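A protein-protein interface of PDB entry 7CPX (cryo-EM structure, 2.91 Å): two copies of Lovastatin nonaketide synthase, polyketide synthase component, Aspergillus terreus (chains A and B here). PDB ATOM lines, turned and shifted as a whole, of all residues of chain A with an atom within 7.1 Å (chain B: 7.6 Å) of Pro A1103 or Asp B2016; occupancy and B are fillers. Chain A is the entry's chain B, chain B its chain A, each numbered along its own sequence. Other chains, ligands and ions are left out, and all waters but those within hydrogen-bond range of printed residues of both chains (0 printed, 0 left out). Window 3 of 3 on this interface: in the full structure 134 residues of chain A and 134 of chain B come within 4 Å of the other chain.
No position is printed for both chains.
Of the 22 pairs that touch across the chains among the printed residues, none has its exchanged pair printed and touching as well.
Pro A1103 touches just these residues of chain B: His B2013 (3.6 Å), Ala B2014 (3.9 Å) and Asp B2016 (2.9 Å).
Asp B2016 touches just these residues of chain A: Pro A1103 (2.9 Å), Arg A1203 (3.5 Å) and Glu A1254 (3.9 Å).
Of the printed residues of chain A, His B2020 touches Glu A1106.
Of the printed residues of chain B, Asp A1239 touches Thr B2017 (3.5 Å), Asp B2018 (3.5 Å) and Trp B2019 (3.7 Å).
Of the printed residues of chain B, Glu A1254 touches Asp B2016, Thr B2017, Asp B2018 and Arg B2047.
Thr B2011 touches none of the printed residues of chain A.
The nearest residue of chain B that does not touch Pro A1103 is Arg B2015 (4.4 Å).
The nearest residue of chain A that does not touch Asp B2016 is Gln A1252 (4.7 Å).
Of the 18 printed residues of chain B, 9 touch a printed residue of chain A.
Along chain B the printed residues that touch a printed residue of chain A span positions 2013 to 2047.
His A1101 touches Arg B2015.
Pro A1103 touches His B2013 (N to ND1, 3.6 Å).
CB of Pro A1103 touches OD1 of Asp B2016, 2.9 Å away.
CZ3 of Trp B2019 touches OE2 of Glu A1106, 3.97 Å away.
NH2 of Arg A1203 touches C of Asp B2016, at 3.5 Å.
N of Thr B2017 touches NH2 of Arg A1203, at 3.6 Å.
Thr A1205 touches Arg B2015 (CG2 to CD, 3.7 Å).
Thr B2017 touches Asp A1239.
Asp B2018 touches Asp A1239.
Asp A1239 touches Trp B2019.
O of Asp B2016 sits at hydrogen-bond distance from NH1 of Arg B2047, at 2.8 Å.
The backbone NH (N) of His B2020 lies within hydrogen-bond range of the side-chain hydroxyl (OG1) of Thr B2017 (3.1 Å).
The backbone carbonyl oxygen (O) of Gly B2043 is in hydrogen-bond range of the guanidinium group (NE) of Arg B2047 (3.3 Å).
The side-chain hydroxyl of Thr A1249 is in hydrogen-bond range of the backbone carbonyl oxygen of Pro A1103, at 2.7 Å.
The guanidinium group (NH2) of Arg A1203 is in salt-bridge range of the side-chain carboxylate (OE1) of Glu A1254, at 2.5 Å.
The backbone NH (N) of Gln A1252 lies within hydrogen-bond range of the backbone carbonyl oxygen (O) of Thr A1205, 2.8 Å away.
NE2 of His B2013 sits at hydrogen-bond distance from O of His A1100, at 2.8 Å.
O of Arg B2015 lies within hydrogen-bond range of NH2 of Arg A1203.
The backbone carbonyl oxygen of Arg B2015 lies close to the side-chain amide oxygen of Gln A1252, at 2.6 Å.
N of Asp B2018 is in hydrogen-bond range of OE2 of Glu A1254.
A ring nitrogen (ND1) of His B2020 sits at hydrogen-bond distance from the side-chain carboxylate of Glu A1106 (2.7 Å).
The guanidinium group (NH1) of Arg B2047 is in salt-bridge range of the side-chain carboxylate (OE1) of Glu A1254.
The guanidinium group (NH1) of Arg B2047 lies close to the guanidinium group (NE) of Arg A1203 (2.8 Å).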
ATOM      1  N   HIS A1100       9.290  11.023  -3.482  1.00  0.00           N
ATOM      2  CA  HIS A1100      10.686  10.951  -3.070  1.00  0.00           C
ATOM      3  C   HIS A1100      10.928   9.760  -2.150  1.00  0.00           C
ATOM      4  O   HIS A1100      11.979   9.656  -1.518  1.00  0.00           O
ATOM      5  CB  HIS A1100      11.103  12.244  -2.369  1.00  0.00           C
ATOM      6  CG  HIS A1100      10.407  12.472  -1.064  1.00  0.00           C
ATOM      7  ND1 HIS A1100       9.073  12.810  -0.980  1.00  0.00           N
ATOM      8  CD2 HIS A1100      10.860  12.410   0.211  1.00  0.00           C
ATOM      9  CE1 HIS A1100       8.734  12.946   0.291  1.00  0.00           C
ATOM     10  NE2 HIS A1100       9.801  12.709   1.033  1.00  0.00           N
ATOM     11  N   HIS A1101       9.947   8.857  -2.076  1.00  0.00           N
ATOM     12  CA  HIS A1101      10.086   7.675  -1.238  1.00  0.00           C
ATOM     13  C   HIS A1101      11.132   6.709  -1.779  1.00  0.00           C
ATOM     14  O   HIS A1101      11.522   5.777  -1.069  1.00  0.00           O
ATOM     15  CB  HIS A1101       8.740   6.963  -1.106  1.00  0.00           C
ATOM     16  CG  HIS A1101       7.640   7.842  -0.598  1.00  0.00           C
ATOM     17  ND1 HIS A1101       7.500   8.163   0.735  1.00  0.00           N
ATOM     18  CD2 HIS A1101       6.629   8.468  -1.245  1.00  0.00           C
ATOM     19  CE1 HIS A1101       6.449   8.950   0.887  1.00  0.00           C
ATOM     20  NE2 HIS A1101       5.903   9.150  -0.298  1.00  0.00           N
ATOM     21  N   LEU A1102      11.588   6.912  -3.013  1.00  0.00           N
ATOM     22  CA  LEU A1102      12.617   6.093  -3.628  1.00  0.00           C
ATOM     23  C   LEU A1102      13.778   6.965  -4.087  1.00  0.00           C
ATOM     24  O   LEU A1102      13.595   8.156  -4.356  1.00  0.00           O
ATOM     25  CB  LEU A1102      12.063   5.316  -4.828  1.00  0.00           C
ATOM     26  CG  LEU A1102      11.363   3.996  -4.515  1.00  0.00           C
ATOM     27  CD1 LEU A1102      10.680   3.443  -5.748  1.00  0.00           C
ATOM     28  CD2 LEU A1102      12.361   2.992  -3.984  1.00  0.00           C
ATOM     29  N   PRO A1103      14.981   6.406  -4.187  1.00  0.00           N
ATOM     30  CA  PRO A1103      16.131   7.201  -4.611  1.00  0.00           C
ATOM     31  C   PRO A1103      15.916   7.761  -6.005  1.00  0.00           C
ATOM     32  O   PRO A1103      15.331   7.089  -6.867  1.00  0.00           O
ATOM     33  CB  PRO A1103      17.289   6.193  -4.587  1.00  0.00           C
ATOM     34  CG  PRO A1103      16.643   4.866  -4.693  1.00  0.00           C
ATOM     35  CD  PRO A1103      15.339   4.995  -3.977  1.00  0.00           C
ATOM     36  N   PRO A1104      16.368   8.986  -6.268  1.00  0.00           N
ATOM     37  CA  PRO A1104      16.272   9.510  -7.622  1.00  0.00           C
ATOM     38  C   PRO A1104      17.065   8.645  -8.583  1.00  0.00           C
ATOM     39  O   PRO A1104      18.101   8.064  -8.213  1.00  0.00           O
ATOM     40  CB  PRO A1104      16.873  10.918  -7.501  1.00  0.00           C
ATOM     41  CG  PRO A1104      16.712  11.277  -6.078  1.00  0.00           C
ATOM     42  CD  PRO A1104      16.875   9.996  -5.325  1.00  0.00           C
ATOM     43  N   PRO A1105      16.613   8.529  -9.827  1.00  0.00           N
ATOM     44  CA  PRO A1105      17.330   7.690 -10.789  1.00  0.00           C
ATOM     45  C   PRO A1105      18.694   8.264 -11.120  1.00  0.00           C
ATOM     46  O   PRO A1105      18.946   9.463 -10.974  1.00  0.00           O
ATOM     47  CB  PRO A1105      16.411   7.701 -12.015  1.00  0.00           C
ATOM     48  CG  PRO A1105      15.713   9.010 -11.920  1.00  0.00           C
ATOM     49  CD  PRO A1105      15.485   9.237 -10.454  1.00  0.00           C
ATOM     50  N   GLU A1106      19.586   7.386 -11.570  1.00  0.00           N
ATOM     51  CA  GLU A1106      20.902   7.829 -11.986  1.00  0.00           C
ATOM     52  C   GLU A1106      20.773   8.820 -13.141  1.00  0.00           C
ATOM     53  O   GLU A1106      19.701   9.015 -13.719  1.00  0.00           O
ATOM     54  CB  GLU A1106      21.768   6.637 -12.388  1.00  0.00           C
ATOM     55  CG  GLU A1106      22.021   5.648 -11.257  1.00  0.00           C
ATOM     56  CD  GLU A1106      22.783   6.263 -10.098  1.00  0.00           C
ATOM     57  OE1 GLU A1106      23.335   7.370 -10.265  1.00  0.00           O
ATOM     58  OE2 GLU A1106      22.828   5.638  -9.017  1.00  0.00           O
ATOM     59  N   ARG A1203      15.028  -7.430  -4.647  1.00  0.00           N
ATOM     60  CA  ARG A1203      14.136  -6.425  -4.074  1.00  0.00           C
ATOM     61  C   ARG A1203      13.494  -5.582  -5.167  1.00  0.00           C
ATOM     62  O   ARG A1203      14.164  -4.749  -5.774  1.00  0.00           O
ATOM     63  CB  ARG A1203      14.888  -5.538  -3.091  1.00  0.00           C
ATOM     64  CG  ARG A1203      14.036  -4.419  -2.511  1.00  0.00           C
ATOM     65  CD  ARG A1203      14.834  -3.545  -1.572  1.00  0.00           C
ATOM     66  NE  ARG A1203      15.952  -2.910  -2.258  1.00  0.00           N
ATOM     67  CZ  ARG A1203      15.845  -1.838  -3.030  1.00  0.00           C
ATOM     68  NH1 ARG A1203      14.676  -1.261  -3.254  1.00  0.00           N
ATOM     69  NH2 ARG A1203      16.938  -1.333  -3.593  1.00  0.00           N
ATOM     70  N   THR A1205      10.687  -2.494  -5.484  1.00  0.00           N
ATOM     71  CA  THR A1205      10.178  -1.470  -4.577  1.00  0.00           C
ATOM     72  C   THR A1205       9.377  -0.463  -5.380  1.00  0.00           C
ATOM     73  O   THR A1205       9.935   0.224  -6.236  1.00  0.00           O
ATOM     74  CB  THR A1205      11.312  -0.780  -3.833  1.00  0.00           C
ATOM     75  OG1 THR A1205      12.141  -1.763  -3.201  1.00  0.00           O
ATOM     76  CG2 THR A1205      10.747   0.141  -2.782  1.00  0.00           C
ATOM     77  N   ASP A1239      19.397  -4.344 -11.929  1.00  0.00           N
ATOM     78  CA  ASP A1239      18.708  -3.389 -11.074  1.00  0.00           C
ATOM     79  C   ASP A1239      18.013  -2.365 -11.955  1.00  0.00           C
ATOM     80  O   ASP A1239      18.657  -1.725 -12.790  1.00  0.00           O
ATOM     81  CB  ASP A1239      19.682  -2.694 -10.122  1.00  0.00           C
ATOM     82  CG  ASP A1239      20.451  -3.672  -9.258  1.00  0.00           C
ATOM     83  OD1 ASP A1239      20.274  -4.894  -9.439  1.00  0.00           O
ATOM     84  OD2 ASP A1239      21.233  -3.219  -8.395  1.00  0.00           O
ATOM     85  N   VAL A1241      15.247   0.989 -12.437  1.00  0.00           N
ATOM     86  CA  VAL A1241      14.687   2.182 -11.819  1.00  0.00           C
ATOM     87  C   VAL A1241      13.798   2.866 -12.845  1.00  0.00           C
ATOM     88  O   VAL A1241      14.291   3.480 -13.797  1.00  0.00           O
ATOM     89  CB  VAL A1241      15.790   3.133 -11.319  1.00  0.00           C
ATOM     90  CG1 VAL A1241      15.183   4.298 -10.557  1.00  0.00           C
ATOM     91  CG2 VAL A1241      16.788   2.389 -10.449  1.00  0.00           C
ATOM     92  N   PHE A1243      10.981   5.751 -13.609  1.00  0.00           N
ATOM     93  CA  PHE A1243      10.648   7.046 -13.039  1.00  0.00           C
ATOM     94  C   PHE A1243       9.755   7.824 -13.995  1.00  0.00           C
ATOM     95  O   PHE A1243       9.641   7.505 -15.181  1.00  0.00           O
ATOM     96  CB  PHE A1243      11.912   7.851 -12.709  1.00  0.00           C
ATOM     97  CG  PHE A1243      12.961   7.809 -13.784  1.00  0.00           C
ATOM     98  CD1 PHE A1243      13.794   6.713 -13.914  1.00  0.00           C
ATOM     99  CD2 PHE A1243      13.129   8.874 -14.649  1.00  0.00           C
ATOM    100  CE1 PHE A1243      14.763   6.673 -14.894  1.00  0.00           C
ATOM    101  CE2 PHE A1243      14.098   8.842 -15.631  1.00  0.00           C
ATOM    102  CZ  PHE A1243      14.917   7.738 -15.755  1.00  0.00           C
ATOM    103  N   GLN A1247      11.031  12.770 -13.170  1.00  0.00           N
ATOM    104  CA  GLN A1247      12.171  12.006 -12.680  1.00  0.00           C
ATOM    105  C   GLN A1247      11.943  11.441 -11.285  1.00  0.00           C
ATOM    106  O   GLN A1247      12.904  11.059 -10.609  1.00  0.00           O
ATOM    107  CB  GLN A1247      13.452  12.846 -12.695  1.00  0.00           C
ATOM    108  CG  GLN A1247      14.726  12.023 -12.754  1.00  0.00           C
ATOM    109  CD  GLN A1247      15.938  12.853 -13.122  1.00  0.00           C
ATOM    110  OE1 GLN A1247      15.955  14.069 -12.933  1.00  0.00           O
ATOM    111  NE2 GLN A1247      16.963  12.197 -13.657  1.00  0.00           N
ATOM    112  N   THR A1248      10.695  11.377 -10.829  1.00  0.00           N
ATOM    113  CA  THR A1248      10.379  10.702  -9.579  1.00  0.00           C
ATOM    114  C   THR A1248      10.262   9.205  -9.830  1.00  0.00           C
ATOM    115  O   THR A1248       9.618   8.777 -10.793  1.00  0.00           O
ATOM    116  CB  THR A1248       9.080  11.241  -8.985  1.00  0.00           C
ATOM    117  OG1 THR A1248       8.057  11.243  -9.988  1.00  0.00           O
ATOM    118  CG2 THR A1248       9.276  12.652  -8.452  1.00  0.00           C
ATOM    119  N   THR A1249      10.880   8.411  -8.962  1.00  0.00           N
ATOM    120  CA  THR A1249      10.959   6.968  -9.159  1.00  0.00           C
ATOM    121  C   THR A1249       9.623   6.333  -8.795  1.00  0.00           C
ATOM    122  O   THR A1249       9.259   6.264  -7.617  1.00  0.00           O
ATOM    123  CB  THR A1249      12.089   6.377  -8.324  1.00  0.00           C
ATOM    124  OG1 THR A1249      13.321   7.037  -8.643  1.00  0.00           O
ATOM    125  CG2 THR A1249      12.231   4.894  -8.602  1.00  0.00           C
ATOM    126  N   GLN A1252      11.489   0.670  -8.582  1.00  0.00           N
ATOM    127  CA  GLN A1252      12.829   0.223  -8.915  1.00  0.00           C
ATOM    128  C   GLN A1252      12.945  -1.266  -8.632  1.00  0.00           C
ATOM    129  O   GLN A1252      12.118  -1.855  -7.931  1.00  0.00           O
ATOM    130  CB  GLN A1252      13.898   0.985  -8.118  1.00  0.00           C
ATOM    131  CG  GLN A1252      13.822   0.779  -6.611  1.00  0.00           C
ATOM    132  CD  GLN A1252      15.097   1.183  -5.898  1.00  0.00           C
ATOM    133  OE1 GLN A1252      15.482   0.568  -4.904  1.00  0.00           O
ATOM    134  NE2 GLN A1252      15.759   2.219  -6.399  1.00  0.00           N
ATOM    135  N   GLU A1254      16.091  -4.368  -7.787  1.00  0.00           N
ATOM    136  CA  GLU A1254      17.451  -4.616  -7.335  1.00  0.00           C
ATOM    137  C   GLU A1254      17.723  -6.106  -7.439  1.00  0.00           C
ATOM    138  O   GLU A1254      17.035  -6.913  -6.801  1.00  0.00           O
ATOM    139  CB  GLU A1254      17.659  -4.135  -5.897  1.00  0.00           C
ATOM    140  CG  GLU A1254      19.032  -4.469  -5.329  1.00  0.00           C
ATOM    141  CD  GLU A1254      19.185  -4.056  -3.882  1.00  0.00           C
ATOM    142  OE1 GLU A1254      18.223  -3.501  -3.313  1.00  0.00           O
ATOM    143  OE2 GLU A1254      20.273  -4.290  -3.314  1.00  0.00           O
ATOM    144  N   THR B1993      23.750  10.065   5.004  1.00  0.00           N
ATOM    145  CA  THR B1993      22.437  10.447   5.499  1.00  0.00           C
ATOM    146  C   THR B1993      21.373  10.035   4.495  1.00  0.00           C
ATOM    147  O   THR B1993      21.557  10.185   3.284  1.00  0.00           O
ATOM    148  CB  THR B1993      22.349  11.958   5.757  1.00  0.00           C
ATOM    149  OG1 THR B1993      21.060  12.279   6.292  1.00  0.00           O
ATOM    150  CG2 THR B1993      22.567  12.737   4.470  1.00  0.00           C
ATOM    151  N   THR B1994      20.262   9.513   5.008  1.00  0.00           N
ATOM    152  CA  THR B1994      19.131   9.107   4.187  1.00  0.00           C
ATOM    153  C   THR B1994      18.056  10.182   4.107  1.00  0.00           C
ATOM    154  O   THR B1994      16.994   9.943   3.523  1.00  0.00           O
ATOM    155  CB  THR B1994      18.526   7.811   4.731  1.00  0.00           C
ATOM    156  OG1 THR B1994      18.061   8.020   6.070  1.00  0.00           O
ATOM    157  CG2 THR B1994      19.561   6.702   4.725  1.00  0.00           C
ATOM    158  N   THR B2011      24.673  11.819   0.819  1.00  0.00           N
ATOM    159  CA  THR B2011      23.212  11.799   0.851  1.00  0.00           C
ATOM    160  C   THR B2011      22.716  10.535   0.157  1.00  0.00           C
ATOM    161  O   THR B2011      22.321  10.533  -1.011  1.00  0.00           O
ATOM    162  CB  THR B2011      22.641  13.050   0.194  1.00  0.00           C
ATOM    163  OG1 THR B2011      23.177  13.187  -1.127  1.00  0.00           O
ATOM    164  CG2 THR B2011      22.983  14.288   1.013  1.00  0.00           C
ATOM    165  N   LEU B2012      22.740   9.433   0.902  1.00  0.00           N
ATOM    166  CA  LEU B2012      22.177   8.183   0.427  1.00  0.00           C
ATOM    167  C   LEU B2012      20.656   8.238   0.518  1.00  0.00           C
ATOM    168  O   LEU B2012      20.058   9.265   0.852  1.00  0.00           O
ATOM    169  CB  LEU B2012      22.726   7.008   1.232  1.00  0.00           C
ATOM    170  CG  LEU B2012      24.239   6.801   1.204  1.00  0.00           C
ATOM    171  CD1 LEU B2012      24.618   5.619   2.075  1.00  0.00           C
ATOM    172  CD2 LEU B2012      24.731   6.593  -0.217  1.00  0.00           C
ATOM    173  N   HIS B2013      20.017   7.113   0.216  1.00  0.00           N
ATOM    174  CA  HIS B2013      18.572   6.994   0.306  1.00  0.00           C
ATOM    175  C   HIS B2013      18.224   5.584   0.746  1.00  0.00           C
ATOM    176  O   HIS B2013      18.883   4.621   0.342  1.00  0.00           O
ATOM    177  CB  HIS B2013      17.898   7.302  -1.034  1.00  0.00           C
ATOM    178  CG  HIS B2013      16.430   7.567  -0.927  1.00  0.00           C
ATOM    179  ND1 HIS B2013      15.516   6.585  -0.610  1.00  0.00           N
ATOM    180  CD2 HIS B2013      15.714   8.703  -1.101  1.00  0.00           C
ATOM    181  CE1 HIS B2013      14.302   7.105  -0.588  1.00  0.00           C
ATOM    182  NE2 HIS B2013      14.395   8.390  -0.883  1.00  0.00           N
ATOM    183  N   ALA B2014      17.191   5.465   1.572  1.00  0.00           N
ATOM    184  CA  ALA B2014      16.717   4.148   1.957  1.00  0.00           C
ATOM    185  C   ALA B2014      16.247   3.392   0.722  1.00  0.00           C
ATOM    186  O   ALA B2014      15.806   3.986  -0.266  1.00  0.00           O
ATOM    187  CB  ALA B2014      15.586   4.262   2.977  1.00  0.00           C
ATOM    188  N   ARG B2015      16.366   2.068   0.777  1.00  0.00           N
ATOM    189  CA  ARG B2015      16.026   1.182  -0.331  1.00  0.00           C
ATOM    190  C   ARG B2015      16.963   1.353  -1.522  1.00  0.00           C
ATOM    191  O   ARG B2015      16.622   0.955  -2.639  1.00  0.00           O
ATOM    192  CB  ARG B2015      14.573   1.379  -0.776  1.00  0.00           C
ATOM    193  CG  ARG B2015      13.554   0.849   0.215  1.00  0.00           C
ATOM    194  CD  ARG B2015      12.276   1.666   0.190  1.00  0.00           C
ATOM    195  NE  ARG B2015      12.352   2.826   1.071  1.00  0.00           N
ATOM    196  CZ  ARG B2015      12.111   2.792   2.374  1.00  0.00           C
ATOM    197  NH1 ARG B2015      11.790   1.666   2.990  1.00  0.00           N
ATOM    198  NH2 ARG B2015      12.195   3.917   3.079  1.00  0.00           N
ATOM    199  N   ASP B2016      18.138   1.939  -1.311  1.00  0.00           N
ATOM    200  CA  ASP B2016      19.119   2.051  -2.380  1.00  0.00           C
ATOM    201  C   ASP B2016      19.679   0.680  -2.745  1.00  0.00           C
ATOM    202  O   ASP B2016      19.815  -0.209  -1.900  1.00  0.00           O
ATOM    203  CB  ASP B2016      20.260   2.982  -1.970  1.00  0.00           C
ATOM    204  CG  ASP B2016      20.038   4.412  -2.417  1.00  0.00           C
ATOM    205  OD1 ASP B2016      19.534   4.612  -3.541  1.00  0.00           O
ATOM    206  OD2 ASP B2016      20.371   5.337  -1.648  1.00  0.00           O
ATOM    207  N   THR B2017      20.005   0.518  -4.024  1.00  0.00           N
ATOM    208  CA  THR B2017      20.514  -0.754  -4.511  1.00  0.00           C
ATOM    209  C   THR B2017      21.958  -0.964  -4.073  1.00  0.00           C
ATOM    210  O   THR B2017      22.712  -0.011  -3.857  1.00  0.00           O
ATOM    211  CB  THR B2017      20.428  -0.820  -6.035  1.00  0.00           C
ATOM    212  OG1 THR B2017      21.359   0.107  -6.607  1.00  0.00           O
ATOM    213  CG2 THR B2017      19.027  -0.478  -6.504  1.00  0.00           C
ATOM    214  N   ASP B2018      22.344  -2.235  -3.952  1.00  0.00           N
ATOM    215  CA  ASP B2018      23.715  -2.554  -3.571  1.00  0.00           C
ATOM    216  C   ASP B2018      24.711  -2.051  -4.606  1.00  0.00           C
ATOM    217  O   ASP B2018      25.819  -1.637  -4.251  1.00  0.00           O
ATOM    218  CB  ASP B2018      23.869  -4.062  -3.377  1.00  0.00           C
ATOM    219  CG  ASP B2018      23.566  -4.845  -4.637  1.00  0.00           C
ATOM    220  OD1 ASP B2018      22.737  -4.376  -5.445  1.00  0.00           O
ATOM    221  OD2 ASP B2018      24.158  -5.929  -4.821  1.00  0.00           O
ATOM    222  N   TRP B2019      24.342  -2.089  -5.888  1.00  0.00           N
ATOM    223  CA  TRP B2019      25.231  -1.579  -6.927  1.00  0.00           C
ATOM    224  C   TRP B2019      25.481  -0.087  -6.750  1.00  0.00           C
ATOM    225  O   TRP B2019      26.617   0.384  -6.891  1.00  0.00           O
ATOM    226  CB  TRP B2019      24.633  -1.864  -8.303  1.00  0.00           C
ATOM    227  CG  TRP B2019      25.394  -1.248  -9.427  1.00  0.00           C
ATOM    228  CD1 TRP B2019      26.394  -1.823 -10.151  1.00  0.00           C
ATOM    229  CD2 TRP B2019      25.217   0.069  -9.960  1.00  0.00           C
ATOM    230  NE1 TRP B2019      26.853  -0.945 -11.103  1.00  0.00           N
ATOM    231  CE2 TRP B2019      26.146   0.224 -11.004  1.00  0.00           C
ATOM    232  CE3 TRP B2019      24.364   1.132  -9.651  1.00  0.00           C
ATOM    233  CZ2 TRP B2019      26.246   1.399 -11.745  1.00  0.00           C
ATOM    234  CZ3 TRP B2019      24.464   2.296 -10.387  1.00  0.00           C
ATOM    235  CH2 TRP B2019      25.398   2.421 -11.422  1.00  0.00           C
ATOM    236  N   HIS B2020      24.431   0.675  -6.438  1.00  0.00           N
ATOM    237  CA  HIS B2020      24.604   2.103  -6.197  1.00  0.00           C
ATOM    238  C   HIS B2020      25.511   2.347  -5.000  1.00  0.00           C
ATOM    239  O   HIS B2020      26.356   3.251  -5.024  1.00  0.00           O
ATOM    240  CB  HIS B2020      23.242   2.764  -5.983  1.00  0.00           C
ATOM    241  CG  HIS B2020      23.327   4.196  -5.558  1.00  0.00           C
ATOM    242  ND1 HIS B2020      23.643   5.215  -6.431  1.00  0.00           N
ATOM    243  CD2 HIS B2020      23.139   4.780  -4.351  1.00  0.00           C
ATOM    244  CE1 HIS B2020      23.643   6.365  -5.780  1.00  0.00           C
ATOM    245  NE2 HIS B2020      23.341   6.128  -4.516  1.00  0.00           N
ATOM    246  N   LEU B2021      25.344   1.555  -3.939  1.00  0.00           N
ATOM    247  CA  LEU B2021      26.207   1.695  -2.773  1.00  0.00           C
ATOM    248  C   LEU B2021      27.658   1.402  -3.128  1.00  0.00           C
ATOM    249  O   LEU B2021      28.567   2.128  -2.709  1.00  0.00           O
ATOM    250  CB  LEU B2021      25.728   0.767  -1.658  1.00  0.00           C
ATOM    251  CG  LEU B2021      24.304   1.036  -1.166  1.00  0.00           C
ATOM    252  CD1 LEU B2021      23.849  -0.062  -0.226  1.00  0.00           C
ATOM    253  CD2 LEU B2021      24.212   2.393  -0.488  1.00  0.00           C
ATOM    254  N   VAL B2024      28.993   4.487  -4.882  1.00  0.00           N
ATOM    255  CA  VAL B2024      29.150   5.710  -4.103  1.00  0.00           C
ATOM    256  C   VAL B2024      29.944   5.475  -2.824  1.00  0.00           C
ATOM    257  O   VAL B2024      30.797   6.290  -2.470  1.00  0.00           O
ATOM    258  CB  VAL B2024      27.769   6.327  -3.791  1.00  0.00           C
ATOM    259  CG1 VAL B2024      26.992   6.561  -5.073  1.00  0.00           C
ATOM    260  CG2 VAL B2024      26.984   5.446  -2.835  1.00  0.00           C
ATOM    261  N   GLY B2043      17.576  -2.361   6.228  1.00  0.00           N
ATOM    262  CA  GLY B2043      17.864  -3.097   5.010  1.00  0.00           C
ATOM    263  C   GLY B2043      19.038  -2.504   4.258  1.00  0.00           C
ATOM    264  O   GLY B2043      19.961  -3.218   3.855  1.00  0.00           O
ATOM    265  N   LEU B2044      19.038  -1.179   4.097  1.00  0.00           N
ATOM    266  CA  LEU B2044      20.178  -0.506   3.488  1.00  0.00           C
ATOM    267  C   LEU B2044      21.465  -0.924   4.183  1.00  0.00           C
ATOM    268  O   LEU B2044      22.445  -1.308   3.535  1.00  0.00           O
ATOM    269  CB  LEU B2044      19.987   1.010   3.568  1.00  0.00           C
ATOM    270  CG  LEU B2044      20.790   1.896   2.611  1.00  0.00           C
ATOM    271  CD1 LEU B2044      20.552   3.358   2.941  1.00  0.00           C
ATOM    272  CD2 LEU B2044      22.272   1.583   2.657  1.00  0.00           C
ATOM    273  N   ARG B2047      22.663  -4.185   3.055  1.00  0.00           N
ATOM    274  CA  ARG B2047      23.304  -4.080   1.751  1.00  0.00           C
ATOM    275  C   ARG B2047      24.713  -3.520   1.879  1.00  0.00           C
ATOM    276  O   ARG B2047      25.620  -3.935   1.149  1.00  0.00           O
ATOM    277  CB  ARG B2047      22.458  -3.211   0.825  1.00  0.00           C
ATOM    278  CG  ARG B2047      21.410  -3.990   0.059  1.00  0.00           C
ATOM    279  CD  ARG B2047      20.268  -3.103  -0.386  1.00  0.00           C
ATOM    280  NE  ARG B2047      19.283  -2.906   0.669  1.00  0.00           N
ATOM    281  CZ  ARG B2047      18.151  -2.236   0.511  1.00  0.00           C
ATOM    282  NH1 ARG B2047      17.845  -1.658  -0.638  1.00  0.00           N
ATOM    283  NH2 ARG B2047      17.301  -2.147   1.531  1.00  0.00           N
ATOM    284  N   MET B2048      24.923  -2.589   2.812  1.00  0.00           N
ATOM    285  CA  MET B2048      26.269  -2.071   3.020  1.00  0.00           C
ATOM    286  C   MET B2048      27.223  -3.196   3.396  1.00  0.00           C
ATOM    287  O   MET B2048      28.346  -3.268   2.884  1.00  0.00           O
ATOM    288  CB  MET B2048      26.264  -0.989   4.099  1.00  0.00           C
ATOM    289  CG  MET B2048      25.583   0.302   3.684  1.00  0.00           C
ATOM    290  SD  MET B2048      25.786   1.606   4.911  1.00  0.00           S
ATOM    291  CE  MET B2048      25.240   3.038   3.987  1.00  0.00           C
